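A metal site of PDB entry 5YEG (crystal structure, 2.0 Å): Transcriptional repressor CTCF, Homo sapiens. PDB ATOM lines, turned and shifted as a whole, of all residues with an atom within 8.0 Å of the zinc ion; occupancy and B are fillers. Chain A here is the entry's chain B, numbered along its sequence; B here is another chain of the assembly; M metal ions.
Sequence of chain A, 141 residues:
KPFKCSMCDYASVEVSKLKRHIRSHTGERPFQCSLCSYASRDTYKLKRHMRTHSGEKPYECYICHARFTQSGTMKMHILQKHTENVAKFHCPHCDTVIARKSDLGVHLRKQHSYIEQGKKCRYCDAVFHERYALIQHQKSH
A ring nitrogen (ND1) of His 21 sits at hydrogen-bond distance from OP2 of DG 16 of chain B (2.9 Å). The backbone carbonyl oxygen of Tyr 10 sits at hydrogen-bond distance from the backbone NH of Cys 5, 2.9 Å away. N of Met 7 lies close to SG of Cys 5 (3.3 Å). The backbone NH (N) of Tyr 10 sits close to the side-chain sulfur (SG) of Cys 8, 3.5 Å away.
Within 4 Å of the zinc ion: Cys 5, Cys 8, His 21 and His 25. The nearest printed residue that does not touch the zinc ion is Met 7 (4.2 Å).
The zinc ion is bound by a ring nitrogen (NE2) of His 25 (2.0 Å), a ring nitrogen (NE2) of His 21 (2.2 Å), the side-chain sulfur (SG) of Cys 8 (2.2 Å) and the side-chain sulfur (SG) of Cys 5 (2.4 Å).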
ATOM      1  N   LYS A   4      12.158 -22.674 -24.894  1.00  0.00           N
ATOM      2  CA  LYS A   4      12.984 -21.544 -24.527  1.00  0.00           C
ATOM      3  C   LYS A   4      12.141 -20.481 -23.828  1.00  0.00           C
ATOM      4  O   LYS A   4      11.019 -20.183 -24.257  1.00  0.00           O
ATOM      5  CB  LYS A   4      13.671 -20.937 -25.760  1.00  0.00           C
ATOM      6  N   CYS A   5      12.683 -19.933 -22.743  1.00  0.00           N
ATOM      7  CA  CYS A   5      12.027 -18.832 -22.055  1.00  0.00           C
ATOM      8  C   CYS A   5      12.105 -17.570 -22.901  1.00  0.00           C
ATOM      9  O   CYS A   5      13.133 -17.278 -23.521  1.00  0.00           O
ATOM     10  CB  CYS A   5      12.666 -18.595 -20.684  1.00  0.00           C
ATOM     11  SG  CYS A   5      11.830 -17.292 -19.734  1.00  0.00           S
ATOM     12  N   SER A   6      10.995 -16.834 -22.948  1.00  0.00           N
ATOM     13  CA  SER A   6      10.968 -15.565 -23.674  1.00  0.00           C
ATOM     14  C   SER A   6      11.633 -14.425 -22.910  1.00  0.00           C
ATOM     15  O   SER A   6      12.004 -13.424 -23.527  1.00  0.00           O
ATOM     16  CB  SER A   6       9.526 -15.185 -23.998  1.00  0.00           C
ATOM     17  OG  SER A   6       8.815 -14.878 -22.815  1.00  0.00           O
ATOM     18  N   MET A   7      11.809 -14.557 -21.586  1.00  0.00           N
ATOM     19  CA  MET A   7      12.306 -13.447 -20.780  1.00  0.00           C
ATOM     20  C   MET A   7      13.781 -13.571 -20.401  1.00  0.00           C
ATOM     21  O   MET A   7      14.375 -12.585 -19.964  1.00  0.00           O
ATOM     22  CB  MET A   7      11.471 -13.297 -19.503  1.00  0.00           C
ATOM     23  CG  MET A   7      10.029 -12.928 -19.783  1.00  0.00           C
ATOM     24  SD  MET A   7       9.051 -12.765 -18.290  1.00  0.00           S
ATOM     25  CE  MET A   7       7.736 -13.940 -18.616  1.00  0.00           C
ATOM     26  N   CYS A   8      14.372 -14.758 -20.524  1.00  0.00           N
ATOM     27  CA  CYS A   8      15.808 -14.939 -20.329  1.00  0.00           C
ATOM     28  C   CYS A   8      16.270 -15.993 -21.328  1.00  0.00           C
ATOM     29  O   CYS A   8      15.494 -16.457 -22.170  1.00  0.00           O
ATOM     30  CB  CYS A   8      16.145 -15.294 -18.869  1.00  0.00           C
ATOM     31  SG  CYS A   8      15.530 -16.890 -18.258  1.00  0.00           S
ATOM     32  N   ASP A   9      17.532 -16.395 -21.229  1.00  0.00           N
ATOM     33  CA  ASP A   9      18.048 -17.406 -22.141  1.00  0.00           C
ATOM     34  C   ASP A   9      17.901 -18.831 -21.614  1.00  0.00           C
ATOM     35  O   ASP A   9      18.499 -19.750 -22.178  1.00  0.00           O
ATOM     36  CB  ASP A   9      19.519 -17.130 -22.504  1.00  0.00           C
ATOM     37  CG  ASP A   9      20.380 -16.872 -21.289  1.00  0.00           C
ATOM     38  OD1 ASP A   9      19.979 -17.263 -20.178  1.00  0.00           O
ATOM     39  OD2 ASP A   9      21.464 -16.270 -21.475  1.00  0.00           O
ATOM     40  N   TYR A  10      17.146 -19.037 -20.533  1.00  0.00           N
ATOM     41  CA  TYR A  10      16.939 -20.397 -20.060  1.00  0.00           C
ATOM     42  C   TYR A  10      16.217 -21.195 -21.128  1.00  0.00           C
ATOM     43  O   TYR A  10      15.258 -20.726 -21.741  1.00  0.00           O
ATOM     44  CB  TYR A  10      16.116 -20.417 -18.765  1.00  0.00           C
ATOM     45  CG  TYR A  10      15.666 -21.806 -18.348  1.00  0.00           C
ATOM     46  CD1 TYR A  10      16.460 -22.579 -17.508  1.00  0.00           C
ATOM     47  CD2 TYR A  10      14.451 -22.340 -18.766  1.00  0.00           C
ATOM     48  CE1 TYR A  10      16.053 -23.859 -17.120  1.00  0.00           C
ATOM     49  CE2 TYR A  10      14.044 -23.599 -18.386  1.00  0.00           C
ATOM     50  CZ  TYR A  10      14.846 -24.366 -17.556  1.00  0.00           C
ATOM     51  OH  TYR A  10      14.431 -25.617 -17.167  1.00  0.00           O
ATOM     52  N   ALA A  11      16.669 -22.427 -21.339  1.00  0.00           N
ATOM     53  CA  ALA A  11      16.040 -23.331 -22.287  1.00  0.00           C
ATOM     54  C   ALA A  11      16.099 -24.738 -21.725  1.00  0.00           C
ATOM     55  O   ALA A  11      17.001 -25.082 -20.956  1.00  0.00           O
ATOM     56  CB  ALA A  11      16.724 -23.270 -23.659  1.00  0.00           C
ATOM     57  N   LEU A  18      10.386 -25.885 -18.279  1.00  0.00           N
ATOM     58  CA  LEU A  18      10.211 -24.499 -18.718  1.00  0.00           C
ATOM     59  C   LEU A  18       9.007 -23.873 -18.009  1.00  0.00           C
ATOM     60  O   LEU A  18       9.074 -22.718 -17.545  1.00  0.00           O
ATOM     61  CB  LEU A  18      10.093 -24.452 -20.243  1.00  0.00           C
ATOM     62  CG  LEU A  18       9.946 -23.158 -21.049  1.00  0.00           C
ATOM     63  CD1 LEU A  18       8.527 -22.857 -21.507  1.00  0.00           C
ATOM     64  CD2 LEU A  18      10.566 -21.946 -20.321  1.00  0.00           C
ATOM     65  N   HIS A  21      10.149 -23.020 -14.584  1.00  0.00           N
ATOM     66  CA  HIS A  21      11.064 -21.876 -14.661  1.00  0.00           C
ATOM     67  C   HIS A  21      10.318 -20.551 -14.798  1.00  0.00           C
ATOM     68  O   HIS A  21      10.718 -19.551 -14.190  1.00  0.00           O
ATOM     69  CB  HIS A  21      12.025 -22.057 -15.837  1.00  0.00           C
ATOM     70  CG  HIS A  21      12.768 -20.811 -16.189  1.00  0.00           C
ATOM     71  ND1 HIS A  21      13.924 -20.439 -15.539  1.00  0.00           N
ATOM     72  CD2 HIS A  21      12.525 -19.851 -17.113  1.00  0.00           C
ATOM     73  CE1 HIS A  21      14.371 -19.303 -16.055  1.00  0.00           C
ATOM     74  NE2 HIS A  21      13.540 -18.924 -17.010  1.00  0.00           N
ATOM     75  N   ILE A  22       9.250 -20.511 -15.601  1.00  0.00           N
ATOM     76  CA  ILE A  22       8.549 -19.237 -15.834  1.00  0.00           C
ATOM     77  C   ILE A  22       7.968 -18.677 -14.533  1.00  0.00           C
ATOM     78  O   ILE A  22       7.844 -17.440 -14.374  1.00  0.00           O
ATOM     79  CB  ILE A  22       7.457 -19.437 -16.914  1.00  0.00           C
ATOM     80  CG1 ILE A  22       8.113 -19.546 -18.302  1.00  0.00           C
ATOM     81  CG2 ILE A  22       6.434 -18.306 -16.895  1.00  0.00           C
ATOM     82  CD1 ILE A  22       7.214 -20.140 -19.356  1.00  0.00           C
ATOM     83  N   ARG A  23       7.625 -19.541 -13.586  1.00  0.00           N
ATOM     84  CA  ARG A  23       7.151 -19.065 -12.286  1.00  0.00           C
ATOM     85  C   ARG A  23       8.195 -18.235 -11.560  1.00  0.00           C
ATOM     86  O   ARG A  23       7.832 -17.462 -10.662  1.00  0.00           O
ATOM     87  CB  ARG A  23       6.713 -20.240 -11.420  1.00  0.00           C
ATOM     88  CG  ARG A  23       5.504 -20.965 -11.964  1.00  0.00           C
ATOM     89  CD  ARG A  23       5.052 -22.086 -11.047  1.00  0.00           C
ATOM     90  NE  ARG A  23       4.354 -23.104 -11.814  1.00  0.00           N
ATOM     91  CZ  ARG A  23       4.680 -24.381 -11.810  1.00  0.00           C
ATOM     92  NH1 ARG A  23       5.683 -24.817 -11.063  1.00  0.00           N
ATOM     93  NH2 ARG A  23       3.988 -25.235 -12.563  1.00  0.00           N
ATOM     94  N   SER A  24       9.471 -18.358 -11.919  1.00  0.00           N
ATOM     95  CA  SER A  24      10.467 -17.461 -11.329  1.00  0.00           C
ATOM     96  C   SER A  24      10.288 -16.036 -11.841  1.00  0.00           C
ATOM     97  O   SER A  24      10.626 -15.083 -11.129  1.00  0.00           O
ATOM     98  CB  SER A  24      11.882 -17.956 -11.592  1.00  0.00           C
ATOM     99  OG  SER A  24      12.199 -19.045 -10.747  1.00  0.00           O
ATOM    100  N   HIS A  25       9.740 -15.873 -13.046  1.00  0.00           N
ATOM    101  CA  HIS A  25       9.434 -14.532 -13.546  1.00  0.00           C
ATOM    102  C   HIS A  25       8.096 -14.027 -13.011  1.00  0.00           C
ATOM    103  O   HIS A  25       7.992 -12.869 -12.570  1.00  0.00           O
ATOM    104  CB  HIS A  25       9.423 -14.535 -15.080  1.00  0.00           C
ATOM    105  CG  HIS A  25      10.761 -14.844 -15.680  1.00  0.00           C
ATOM    106  ND1 HIS A  25      11.848 -14.005 -15.548  1.00  0.00           N
ATOM    107  CD2 HIS A  25      11.195 -15.903 -16.403  1.00  0.00           C
ATOM    108  CE1 HIS A  25      12.885 -14.523 -16.169  1.00  0.00           C
ATOM    109  NE2 HIS A  25      12.525 -15.678 -16.693  1.00  0.00           N
ATOM    110  P    DG B  16      16.652 -21.461 -13.190  1.00  0.00           P
ATOM    111  OP1  DG B  16      17.322 -20.599 -14.194  1.00  0.00           O
ATOM    112  OP2  DG B  16      15.207 -21.730 -13.321  1.00  0.00           O
ATOM    113  O5'  DG B  16      17.372 -22.867 -13.139  1.00  0.00           O
ATOM    114  C5'  DG B  16      18.756 -22.938 -13.067  1.00  0.00           C
ATOM    115  C4'  DG B  16      19.208 -24.366 -13.088  1.00  0.00           C
ATOM    116  O4'  DG B  16      18.877 -24.994 -11.825  1.00  0.00           O
ATOM    117  C3'  DG B  16      18.568 -25.220 -14.181  1.00  0.00           C
ATOM    118  O3'  DG B  16      19.564 -25.935 -14.828  1.00  0.00           O
ATOM    119  C2'  DG B  16      17.630 -26.148 -13.414  1.00  0.00           C
ATOM    120  C1'  DG B  16      18.337 -26.271 -12.075  1.00  0.00           C
ATOM    121  N9   DG B  16      17.440 -26.610 -10.983  1.00  0.00           N
ATOM    122  C8   DG B  16      16.307 -25.921 -10.600  1.00  0.00           C
ATOM    123  N7   DG B  16      15.694 -26.459  -9.592  1.00  0.00           N
ATOM    124  C5   DG B  16      16.467 -27.578  -9.281  1.00  0.00           C
ATOM    125  C6   DG B  16      16.300 -28.549  -8.256  1.00  0.00           C
ATOM    126  O6   DG B  16      15.397 -28.616  -7.406  1.00  0.00           O
ATOM    127  N1   DG B  16      17.309 -29.517  -8.300  1.00  0.00           N
ATOM    128  C2   DG B  16      18.350 -29.532  -9.195  1.00  0.00           C
ATOM    129  N2   DG B  16      19.230 -30.540  -9.074  1.00  0.00           N
ATOM    130  N3   DG B  16      18.522 -28.621 -10.138  1.00  0.00           N
ATOM    131  C4   DG B  16      17.543 -27.685 -10.130  1.00  0.00           C
HETATM  132 ZN    ZN M   1      13.328 -16.988 -17.948  1.00  0.00          ZN
